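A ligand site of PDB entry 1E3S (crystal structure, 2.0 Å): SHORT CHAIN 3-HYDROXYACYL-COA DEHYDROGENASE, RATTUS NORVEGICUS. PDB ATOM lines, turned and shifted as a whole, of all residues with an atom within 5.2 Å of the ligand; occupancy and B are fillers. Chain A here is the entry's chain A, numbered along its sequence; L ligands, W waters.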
ATOM      1  N   GLY A  17      34.132 -19.618 -11.769  1.00  0.00           N
ATOM      2  CA  GLY A  17      32.773 -19.934 -11.329  1.00  0.00           C
ATOM      3  C   GLY A  17      32.040 -20.726 -12.421  1.00  0.00           C
ATOM      4  O   GLY A  17      30.806 -20.848 -12.447  1.00  0.00           O
ATOM      5  N   ALA A  19      31.455 -24.011 -12.754  1.00  0.00           N
ATOM      6  CA  ALA A  19      30.746 -25.251 -12.435  1.00  0.00           C
ATOM      7  C   ALA A  19      29.256 -25.068 -12.233  1.00  0.00           C
ATOM      8  O   ALA A  19      28.515 -26.063 -12.147  1.00  0.00           O
ATOM      9  CB  ALA A  19      31.337 -25.839 -11.146  1.00  0.00           C
ATOM     10  N   SER A  20      28.761 -23.836 -12.130  1.00  0.00           N
ATOM     11  CA  SER A  20      27.373 -23.536 -11.838  1.00  0.00           C
ATOM     12  C   SER A  20      26.852 -22.227 -12.420  1.00  0.00           C
ATOM     13  O   SER A  20      27.618 -21.372 -12.861  1.00  0.00           O
ATOM     14  CB  SER A  20      27.278 -23.404 -10.289  1.00  0.00           C
ATOM     15  OG  SER A  20      25.890 -23.274  -9.948  1.00  0.00           O
ATOM     16  N   GLY A  21      25.540 -22.017 -12.409  1.00  0.00           N
ATOM     17  CA  GLY A  21      24.857 -20.812 -12.795  1.00  0.00           C
ATOM     18  C   GLY A  21      25.325 -20.084 -14.045  1.00  0.00           C
ATOM     19  O   GLY A  21      25.339 -20.664 -15.118  1.00  0.00           O
ATOM     20  N   LEU A  22      25.638 -18.771 -13.928  1.00  0.00           N
ATOM     21  CA  LEU A  22      26.033 -17.983 -15.084  1.00  0.00           C
ATOM     22  C   LEU A  22      27.333 -18.445 -15.767  1.00  0.00           C
ATOM     23  O   LEU A  22      27.392 -18.439 -17.000  1.00  0.00           O
ATOM     24  CB  LEU A  22      26.204 -16.497 -14.696  1.00  0.00           C
ATOM     25  CG  LEU A  22      24.995 -15.842 -14.004  1.00  0.00           C
ATOM     26  CD1 LEU A  22      25.254 -14.379 -13.726  1.00  0.00           C
ATOM     27  CD2 LEU A  22      23.695 -16.018 -14.844  1.00  0.00           C
ATOM     28  N   GLY A  23      28.328 -18.850 -14.971  1.00  0.00           N
ATOM     29  CA  GLY A  23      29.546 -19.335 -15.647  1.00  0.00           C
ATOM     30  C   GLY A  23      29.273 -20.654 -16.384  1.00  0.00           C
ATOM     31  O   GLY A  23      29.845 -20.851 -17.471  1.00  0.00           O
ATOM     32  N   LEU A  40      37.137 -22.953 -14.193  1.00  0.00           N
ATOM     33  CA  LEU A  40      37.933 -22.744 -12.990  1.00  0.00           C
ATOM     34  C   LEU A  40      36.981 -22.584 -11.805  1.00  0.00           C
ATOM     35  O   LEU A  40      36.152 -21.663 -11.809  1.00  0.00           O
ATOM     36  CB  LEU A  40      38.881 -21.555 -13.179  1.00  0.00           C
ATOM     37  CG  LEU A  40      39.985 -21.258 -12.172  1.00  0.00           C
ATOM     38  CD1 LEU A  40      41.083 -20.392 -12.795  1.00  0.00           C
ATOM     39  CD2 LEU A  40      39.429 -20.515 -10.954  1.00  0.00           C
ATOM     40  N   ASP A  41      37.031 -23.520 -10.844  1.00  0.00           N
ATOM     41  CA  ASP A  41      36.127 -23.529  -9.702  1.00  0.00           C
ATOM     42  C   ASP A  41      36.727 -24.402  -8.585  1.00  0.00           C
ATOM     43  O   ASP A  41      37.845 -24.951  -8.722  1.00  0.00           O
ATOM     44  CB  ASP A  41      34.719 -24.023 -10.096  1.00  0.00           C
ATOM     45  CG  ASP A  41      33.562 -23.449  -9.325  1.00  0.00           C
ATOM     46  OD1 ASP A  41      33.437 -23.554  -8.081  1.00  0.00           O
ATOM     47  OD2 ASP A  41      32.579 -22.900  -9.938  1.00  0.00           O
ATOM     48  N   VAL A  42      36.150 -24.287  -7.389  1.00  0.00           N
ATOM     49  CA  VAL A  42      36.737 -25.010  -6.249  1.00  0.00           C
ATOM     50  C   VAL A  42      36.578 -26.527  -6.364  1.00  0.00           C
ATOM     51  O   VAL A  42      35.653 -27.073  -6.989  1.00  0.00           O
ATOM     52  CB  VAL A  42      36.188 -24.489  -4.920  1.00  0.00           C
ATOM     53  CG1 VAL A  42      36.490 -22.989  -4.781  1.00  0.00           C
ATOM     54  CG2 VAL A  42      34.684 -24.718  -4.826  1.00  0.00           C
ATOM     55  N   SER A  45      33.175 -28.431  -5.868  1.00  0.00           N
ATOM     56  CA  SER A  45      32.071 -28.134  -6.776  1.00  0.00           C
ATOM     57  C   SER A  45      31.852 -29.358  -7.671  1.00  0.00           C
ATOM     58  O   SER A  45      32.668 -30.279  -7.652  1.00  0.00           O
ATOM     59  CB  SER A  45      32.428 -26.912  -7.629  1.00  0.00           C
ATOM     60  OG  SER A  45      33.477 -27.212  -8.526  1.00  0.00           O
ATOM     61  N   ALA A  63      40.710 -24.588  -8.617  1.00  0.00           N
ATOM     62  CA  ALA A  63      41.455 -23.462  -8.117  1.00  0.00           C
ATOM     63  C   ALA A  63      40.557 -22.458  -7.367  1.00  0.00           C
ATOM     64  O   ALA A  63      39.401 -22.287  -7.689  1.00  0.00           O
ATOM     65  CB  ALA A  63      42.170 -22.713  -9.245  1.00  0.00           C
ATOM     66  N   ASN A  64      41.070 -21.914  -6.265  1.00  0.00           N
ATOM     67  CA  ASN A  64      40.382 -20.857  -5.514  1.00  0.00           C
ATOM     68  C   ASN A  64      40.884 -19.542  -6.097  1.00  0.00           C
ATOM     69  O   ASN A  64      42.093 -19.361  -6.123  1.00  0.00           O
ATOM     70  CB  ASN A  64      40.715 -21.000  -4.031  1.00  0.00           C
ATOM     71  CG  ASN A  64      39.831 -20.157  -3.152  1.00  0.00           C
ATOM     72  OD1 ASN A  64      39.846 -18.848  -3.369  1.00  0.00           O
ATOM     73  ND2 ASN A  64      39.125 -20.720  -2.296  1.00  0.00           N
ATOM     74  N   VAL A  65      40.024 -18.614  -6.528  1.00  0.00           N
ATOM     75  CA  VAL A  65      40.500 -17.347  -7.107  1.00  0.00           C
ATOM     76  C   VAL A  65      41.291 -16.452  -6.184  1.00  0.00           C
ATOM     77  O   VAL A  65      41.943 -15.508  -6.680  1.00  0.00           O
ATOM     78  CB  VAL A  65      39.359 -16.539  -7.755  1.00  0.00           C
ATOM     79  CG1 VAL A  65      38.780 -17.319  -8.923  1.00  0.00           C
ATOM     80  CG2 VAL A  65      38.252 -16.214  -6.748  1.00  0.00           C
ATOM     81  N   THR A  66      41.252 -16.644  -4.855  1.00  0.00           N
ATOM     82  CA  THR A  66      42.062 -15.812  -3.980  1.00  0.00           C
ATOM     83  C   THR A  66      43.512 -16.295  -3.864  1.00  0.00           C
ATOM     84  O   THR A  66      44.410 -15.599  -3.327  1.00  0.00           O
ATOM     85  CB  THR A  66      41.497 -15.723  -2.553  1.00  0.00           C
ATOM     86  OG1 THR A  66      41.451 -17.011  -1.942  1.00  0.00           O
ATOM     87  CG2 THR A  66      40.055 -15.193  -2.581  1.00  0.00           C
ATOM     88  N   CYS A  91      33.161 -15.068 -13.217  1.00  0.00           N
ATOM     89  CA  CYS A  91      31.828 -15.315 -12.660  1.00  0.00           C
ATOM     90  C   CYS A  91      31.934 -15.857 -11.223  1.00  0.00           C
ATOM     91  O   CYS A  91      30.924 -15.805 -10.498  1.00  0.00           O
ATOM     92  CB  CYS A  91      30.921 -16.246 -13.471  1.00  0.00           C
ATOM     93  SG  CYS A  91      30.521 -15.737 -15.181  1.00  0.00           S
ATOM     94  N   ALA A  92      33.123 -16.212 -10.713  1.00  0.00           N
ATOM     95  CA  ALA A  92      33.237 -16.678  -9.327  1.00  0.00           C
ATOM     96  C   ALA A  92      32.806 -15.586  -8.336  1.00  0.00           C
ATOM     97  O   ALA A  92      33.310 -14.441  -8.403  1.00  0.00           O
ATOM     98  CB  ALA A  92      34.673 -17.069  -9.036  1.00  0.00           C
ATOM     99  N   GLY A  93      31.938 -15.911  -7.381  1.00  0.00           N
ATOM    100  CA  GLY A  93      31.468 -14.902  -6.423  1.00  0.00           C
ATOM    101  C   GLY A  93      30.596 -15.487  -5.324  1.00  0.00           C
ATOM    102  O   GLY A  93      30.030 -16.587  -5.453  1.00  0.00           O
ATOM    103  N   ILE A  94      30.467 -14.795  -4.185  1.00  0.00           N
ATOM    104  CA  ILE A  94      29.652 -15.191  -3.054  1.00  0.00           C
ATOM    105  C   ILE A  94      28.808 -14.016  -2.577  1.00  0.00           C
ATOM    106  O   ILE A  94      29.052 -12.864  -2.942  1.00  0.00           O
ATOM    107  CB  ILE A  94      30.429 -15.682  -1.800  1.00  0.00           C
ATOM    108  CG1 ILE A  94      31.432 -14.628  -1.330  1.00  0.00           C
ATOM    109  CG2 ILE A  94      31.049 -17.045  -2.070  1.00  0.00           C
ATOM    110  CD1 ILE A  94      32.262 -14.990  -0.086  1.00  0.00           C
ATOM    111  N   VAL A 120      36.968 -12.612  -1.958  1.00  0.00           N
ATOM    112  CA  VAL A 120      36.555 -13.474  -3.063  1.00  0.00           C
ATOM    113  C   VAL A 120      36.084 -12.689  -4.289  1.00  0.00           C
ATOM    114  O   VAL A 120      36.536 -12.928  -5.418  1.00  0.00           O
ATOM    115  CB  VAL A 120      35.414 -14.441  -2.652  1.00  0.00           C
ATOM    116  CG1 VAL A 120      34.825 -15.264  -3.801  1.00  0.00           C
ATOM    117  CG2 VAL A 120      35.810 -15.424  -1.557  1.00  0.00           C
ATOM    118  N   ASN A 121      35.219 -11.695  -4.111  1.00  0.00           N
ATOM    119  CA  ASN A 121      34.583 -10.996  -5.227  1.00  0.00           C
ATOM    120  C   ASN A 121      35.445  -9.961  -5.942  1.00  0.00           C
ATOM    121  O   ASN A 121      35.449  -9.938  -7.186  1.00  0.00           O
ATOM    122  CB  ASN A 121      33.279 -10.286  -4.777  1.00  0.00           C
ATOM    123  CG  ASN A 121      32.160 -11.223  -4.402  1.00  0.00           C
ATOM    124  OD1 ASN A 121      32.335 -12.446  -4.395  1.00  0.00           O
ATOM    125  ND2 ASN A 121      30.960 -10.726  -4.066  1.00  0.00           N
ATOM    126  N   THR A 153      31.983  -9.778 -13.944  1.00  0.00           N
ATOM    127  CA  THR A 153      30.586  -9.785 -13.525  1.00  0.00           C
ATOM    128  C   THR A 153      30.398  -8.931 -12.269  1.00  0.00           C
ATOM    129  O   THR A 153      30.972  -9.276 -11.211  1.00  0.00           O
ATOM    130  CB  THR A 153      29.998 -11.177 -13.238  1.00  0.00           C
ATOM    131  OG1 THR A 153      30.218 -12.089 -14.324  1.00  0.00           O
ATOM    132  CG2 THR A 153      28.459 -11.060 -13.025  1.00  0.00           C
ATOM    133  N   ALA A 154      29.745  -7.761 -12.435  1.00  0.00           N
ATOM    134  CA  ALA A 154      29.419  -6.926 -11.279  1.00  0.00           C
ATOM    135  C   ALA A 154      28.000  -7.246 -10.786  1.00  0.00           C
ATOM    136  O   ALA A 154      27.686  -8.427 -10.512  1.00  0.00           O
ATOM    137  CB  ALA A 154      29.605  -5.437 -11.617  1.00  0.00           C
ATOM    138  N   SER A 155      27.142  -6.258 -10.628  1.00  0.00           N
ATOM    139  CA  SER A 155      25.742  -6.428 -10.219  1.00  0.00           C
ATOM    140  C   SER A 155      24.996  -5.090 -10.272  1.00  0.00           C
ATOM    141  O   SER A 155      25.660  -4.062 -10.090  1.00  0.00           O
ATOM    142  CB  SER A 155      25.663  -6.887  -8.753  1.00  0.00           C
ATOM    143  OG  SER A 155      24.313  -6.836  -8.265  1.00  0.00           O
ATOM    144  N   TYR A 168      28.491  -6.827  -0.204  1.00  0.00           N
ATOM    145  CA  TYR A 168      28.316  -7.191  -1.614  1.00  0.00           C
ATOM    146  C   TYR A 168      28.388  -5.996  -2.540  1.00  0.00           C
ATOM    147  O   TYR A 168      29.117  -6.040  -3.541  1.00  0.00           O
ATOM    148  CB  TYR A 168      26.976  -7.943  -1.782  1.00  0.00           C
ATOM    149  CG  TYR A 168      26.714  -8.564  -3.139  1.00  0.00           C
ATOM    150  CD1 TYR A 168      27.321  -9.758  -3.496  1.00  0.00           C
ATOM    151  CD2 TYR A 168      25.788  -8.002  -4.028  1.00  0.00           C
ATOM    152  CE1 TYR A 168      27.005 -10.397  -4.684  1.00  0.00           C
ATOM    153  CE2 TYR A 168      25.515  -8.623  -5.246  1.00  0.00           C
ATOM    154  CZ  TYR A 168      26.120  -9.805  -5.577  1.00  0.00           C
ATOM    155  OH  TYR A 168      25.870 -10.428  -6.800  1.00  0.00           O
ATOM    156  N   LYS A 172      31.136  -5.157  -5.551  1.00  0.00           N
ATOM    157  CA  LYS A 172      30.705  -4.987  -6.934  1.00  0.00           C
ATOM    158  C   LYS A 172      30.952  -3.554  -7.446  1.00  0.00           C
ATOM    159  O   LYS A 172      31.273  -3.364  -8.633  1.00  0.00           O
ATOM    160  CB  LYS A 172      29.232  -5.411  -7.145  1.00  0.00           C
ATOM    161  CG  LYS A 172      28.918  -6.894  -6.817  1.00  0.00           C
ATOM    162  CD  LYS A 172      29.887  -7.879  -7.500  1.00  0.00           C
ATOM    163  CE  LYS A 172      29.310  -9.306  -7.517  1.00  0.00           C
ATOM    164  NZ  LYS A 172      29.982 -10.238  -8.468  1.00  0.00           N
ATOM    165  N   PRO A 198      24.275  -7.845 -13.918  1.00  0.00           N
ATOM    166  CA  PRO A 198      23.015  -8.547 -13.864  1.00  0.00           C
ATOM    167  C   PRO A 198      22.063  -8.046 -12.775  1.00  0.00           C
ATOM    168  O   PRO A 198      22.493  -7.592 -11.705  1.00  0.00           O
ATOM    169  CB  PRO A 198      23.396 -10.004 -13.572  1.00  0.00           C
ATOM    170  CG  PRO A 198      24.868 -10.081 -13.862  1.00  0.00           C
ATOM    171  CD  PRO A 198      25.415  -8.717 -13.475  1.00  0.00           C
ATOM    172  N   GLY A 199      20.775  -8.072 -13.074  1.00  0.00           N
ATOM    173  CA  GLY A 199      19.703  -7.790 -12.116  1.00  0.00           C
ATOM    174  C   GLY A 199      19.339  -9.134 -11.457  1.00  0.00           C
ATOM    175  O   GLY A 199      20.289  -9.806 -11.062  1.00  0.00           O
ATOM    176  N   LEU A 200      18.131  -9.632 -11.361  1.00  0.00           N
ATOM    177  CA  LEU A 200      17.881 -10.930 -10.694  1.00  0.00           C
ATOM    178  C   LEU A 200      17.755 -12.139 -11.599  1.00  0.00           C
ATOM    179  O   LEU A 200      16.973 -12.044 -12.567  1.00  0.00           O
ATOM    180  CB  LEU A 200      16.574 -10.737  -9.910  1.00  0.00           C
ATOM    181  CG  LEU A 200      16.633  -9.588  -8.887  1.00  0.00           C
ATOM    182  CD1 LEU A 200      15.253  -9.304  -8.313  1.00  0.00           C
ATOM    183  CD2 LEU A 200      17.648  -9.884  -7.789  1.00  0.00           C
ATOM    184  N   PHE A 201      18.621 -13.165 -11.473  1.00  0.00           N
ATOM    185  CA  PHE A 201      18.641 -14.338 -12.324  1.00  0.00           C
ATOM    186  C   PHE A 201      18.335 -15.663 -11.585  1.00  0.00           C
ATOM    187  O   PHE A 201      18.708 -15.900 -10.431  1.00  0.00           O
ATOM    188  CB  PHE A 201      20.003 -14.490 -13.030  1.00  0.00           C
ATOM    189  CG  PHE A 201      20.156 -13.675 -14.290  1.00  0.00           C
ATOM    190  CD1 PHE A 201      20.254 -12.293 -14.241  1.00  0.00           C
ATOM    191  CD2 PHE A 201      20.216 -14.289 -15.525  1.00  0.00           C
ATOM    192  CE1 PHE A 201      20.361 -11.539 -15.405  1.00  0.00           C
ATOM    193  CE2 PHE A 201      20.312 -13.568 -16.697  1.00  0.00           C
ATOM    194  CZ  PHE A 201      20.389 -12.169 -16.641  1.00  0.00           C
ATOM    195  N   THR A 203      19.394 -18.727 -10.634  1.00  0.00           N
ATOM    196  CA  THR A 203      20.543 -19.595 -10.387  1.00  0.00           C
ATOM    197  C   THR A 203      20.521 -20.057  -8.909  1.00  0.00           C
ATOM    198  O   THR A 203      19.768 -19.524  -8.073  1.00  0.00           O
ATOM    199  CB  THR A 203      21.886 -18.856 -10.571  1.00  0.00           C
ATOM    200  OG1 THR A 203      21.961 -17.957  -9.455  1.00  0.00           O
ATOM    201  CG2 THR A 203      22.042 -18.070 -11.841  1.00  0.00           C
ATOM    202  N   PRO A 204      21.408 -20.971  -8.576  1.00  0.00           N
ATOM    203  CA  PRO A 204      21.542 -21.474  -7.211  1.00  0.00           C
ATOM    204  C   PRO A 204      21.979 -20.394  -6.229  1.00  0.00           C
ATOM    205  O   PRO A 204      21.756 -20.515  -5.022  1.00  0.00           O
ATOM    206  CB  PRO A 204      22.599 -22.576  -7.328  1.00  0.00           C
ATOM    207  CG  PRO A 204      22.495 -23.022  -8.751  1.00  0.00           C
ATOM    208  CD  PRO A 204      22.304 -21.711  -9.503  1.00  0.00           C
HETATM  209  P1  LIG L   1      26.469 -19.673  -8.373  1.00  0.00           P
HETATM  210  O1  LIG L   1      26.538 -19.938  -6.927  1.00  0.00           O
HETATM  211  O2  LIG L   1      25.487 -20.564  -9.051  1.00  0.00           O
HETATM  212  O3  LIG L   1      27.872 -19.832  -9.082  1.00  0.00           O
HETATM  213  C1  LIG L   1      29.103 -19.156  -8.642  1.00  0.00           C
HETATM  214  C2  LIG L   1      30.255 -20.151  -8.757  1.00  0.00           C
HETATM  215  O4  LIG L   1      31.467 -19.501  -8.252  1.00  0.00           O
HETATM  216  C3  LIG L   1      30.044 -21.436  -7.930  1.00  0.00           C
HETATM  217  O5  LIG L   1      30.226 -22.585  -8.768  1.00  0.00           O
HETATM  218  C4  LIG L   1      31.133 -21.381  -6.858  1.00  0.00           C
HETATM  219  O6  LIG L   1      31.664 -22.680  -6.514  1.00  0.00           O
HETATM  220  C5  LIG L   1      32.195 -20.471  -7.504  1.00  0.00           C
HETATM  221  N1  LIG L   1      33.076 -19.828  -6.514  1.00  0.00           N
HETATM  222  C6  LIG L   1      32.713 -19.273  -5.300  1.00  0.00           C
HETATM  223  N2  LIG L   1      33.756 -18.871  -4.587  1.00  0.00           N
HETATM  224  C7  LIG L   1      34.862 -19.192  -5.362  1.00  0.00           C
HETATM  225  C8  LIG L   1      36.254 -19.041  -5.161  1.00  0.00           C
HETATM  226  N3  LIG L   1      36.845 -18.460  -4.110  1.00  0.00           N
HETATM  227  N4  LIG L   1      37.062 -19.562  -6.124  1.00  0.00           N
HETATM  228  C9  LIG L   1      36.503 -20.113  -7.241  1.00  0.00           C
HETATM  229  N5  LIG L   1      35.242 -20.305  -7.509  1.00  0.00           N
HETATM  230  C10 LIG L   1      34.445 -19.839  -6.520  1.00  0.00           C
HETATM  231  O7  LIG L   1      26.097 -18.139  -8.591  1.00  0.00           O
HETATM  232  P2  LIG L   1      25.732 -17.276  -9.886  1.00  0.00           P
HETATM  233  O8  LIG L   1      24.346 -16.818  -9.722  1.00  0.00           O
HETATM  234  O9  LIG L   1      26.002 -18.044 -11.123  1.00  0.00           O
HETATM  235  O10 LIG L   1      26.779 -16.067  -9.736  1.00  0.00           O
HETATM  236  C11 LIG L   1      27.794 -15.853 -10.740  1.00  0.00           C
HETATM  237  C12 LIG L   1      28.223 -14.396 -10.590  1.00  0.00           C
HETATM  238  O11 LIG L   1      27.010 -13.625 -10.920  1.00  0.00           O
HETATM  239  C13 LIG L   1      28.615 -13.943  -9.186  1.00  0.00           C
HETATM  240  O12 LIG L   1      29.705 -13.030  -9.286  1.00  0.00           O
HETATM  241  C14 LIG L   1      27.368 -13.204  -8.684  1.00  0.00           C
HETATM  242  O13 LIG L   1      27.693 -12.182  -7.736  1.00  0.00           O
HETATM  243  C15 LIG L   1      26.875 -12.579  -9.993  1.00  0.00           C
HETATM  244  N6  LIG L   1      25.461 -12.185 -10.003  1.00  0.00           N
HETATM  245  C16 LIG L   1      24.507 -13.163  -9.897  1.00  0.00           C
HETATM  246  C17 LIG L   1      23.180 -12.775  -9.907  1.00  0.00           C
HETATM  247  C18 LIG L   1      21.948 -13.710  -9.790  1.00  0.00           C
HETATM  248  O14 LIG L   1      20.849 -13.212  -9.550  1.00  0.00           O
HETATM  249  N7  LIG L   1      22.124 -15.036  -9.968  1.00  0.00           N
HETATM  250  C19 LIG L   1      22.752 -11.422 -10.020  1.00  0.00           C
HETATM  251  C20 LIG L   1      23.818 -10.513 -10.128  1.00  0.00           C
HETATM  252  C21 LIG L   1      25.165 -10.807 -10.144  1.00  0.00           C
HETATM  253  O   HOH W   1      28.692 -18.727 -11.963  1.00  0.00           O
HETATM  254  O   HOH W   2      32.249 -12.746 -10.287  1.00  0.00           O
HETATM  255  O   HOH W   3      29.177 -24.600  -7.147  1.00  0.00           O
HETATM  256  O   HOH W   4      21.772  -8.447  -8.536  1.00  0.00           O
HETATM  257  O   HOH W   5      34.390 -19.151  -1.776  1.00  0.00           O
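The side-chain carboxylate (OD1) of Asp 41 is in hydrogen-bond range of an oxygen (O6) of the ligand (2.5 Å).
An oxygen (O8) of the ligand sits at hydrogen-bond distance from the side-chain hydroxyl (OG1) of Thr 203, at 2.7 Å.
The side-chain hydroxyl (OH) of Tyr 168 sits at hydrogen-bond distance from an oxygen (O13) of the ligand (2.7 Å).
OG of Ser 20 is in hydrogen-bond range of O2 of the ligand, at 2.9 Å.
The backbone NH of Leu 22 sits at hydrogen-bond distance from an oxygen (O9) of the ligand.
The side-chain amino group of Lys 172 is in hydrogen-bond range of an oxygen (O12) of the ligand (2.9 Å).
The backbone NH (N) of Phe 201 sits at hydrogen-bond distance from an oxygen (O14) of the ligand.
The backbone carbonyl oxygen (O) of Cys 91 lies close to an oxygen (O12) of the ligand, at 3.3 Å.
OD1 of Asn 64 sits at hydrogen-bond distance from N3 of the ligand (3.1 Å).
A nitrogen (N4) of the ligand lies within hydrogen-bond range of the backbone NH of Val 65 (3.1 Å).
The backbone carbonyl oxygen (O) of Asp 41 is in hydrogen-bond range of the backbone NH (N) of Ala 63 (2.9 Å).
The backbone NH (N) of Ala 19 lies within hydrogen-bond range of the side-chain carboxylate (OD2) of Asp 41 (3.2 Å).
O of Thr 153 is in hydrogen-bond range of NZ of Lys 172.
The side-chain sulfur of Cys 91 lies within hydrogen-bond range of the side-chain hydroxyl of Thr 153 (3.8 Å).
The side-chain hydroxyl of Thr 66 lies within hydrogen-bond range of the side-chain amide oxygen of Asn 64 (2.8 Å).
The backbone carbonyl oxygen of Leu 40 is in hydrogen-bond range of the backbone NH of Gly 17, at 2.9 Å.
The side-chain hydroxyl of Ser 45 lies within hydrogen-bond range of the backbone carbonyl oxygen of Val 42 (2.7 Å).
CA of Gly 17 touches O4 of the ligand, at 3.4 Å.
CA of Gly 21 touches O9 of the ligand, 3.4 Å away.
Val 42 touches the ligand.
Ala 63 touches the ligand (O to C9, 3.7 Å).
CA of Ala 92 touches O4 of the ligand, at 3.5 Å.
N of Gly 93 touches O4 of the ligand, 3.7 Å away.
Val 120 touches the ligand.
CG2 of Thr 153 touches O11 of the ligand (3.6 Å).
Ala 154 touches the ligand (O to C21, 3.5 Å).
Pro 198 touches the ligand.
O of Gly 199 touches C19 of the ligand (3.1 Å).
C of Leu 200 touches O14 of the ligand, at 3.9 Å.
Pro 204 touches the ligand.
Hydrophobic or aromatic side chains within 4 Å of the ligand: Leu 22, Val 42, Val 65, Ala 92, Val 120, Tyr 168, Pro 198, Phe 201 and Pro 204.
Water W2 lies within hydrogen-bond range of O of Ala 92 (2.7 Å), O12 of the ligand (2.7 Å) and O of Cys 91 (3.3 Å).
Water W1 lies within hydrogen-bond range of O9 of the ligand (2.9 Å), O of Ser 20 (3.0 Å), N of Gly 23 (3.0 Å) and O of Gly 17 (3.0 Å).
Water W4 lies within hydrogen-bond range of the side-chain hydroxyl of Ser 155 (3.0 Å), the backbone carbonyl oxygen of Gly 199 (3.2 Å) and the backbone carbonyl oxygen of Pro 198 (3.4 Å).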
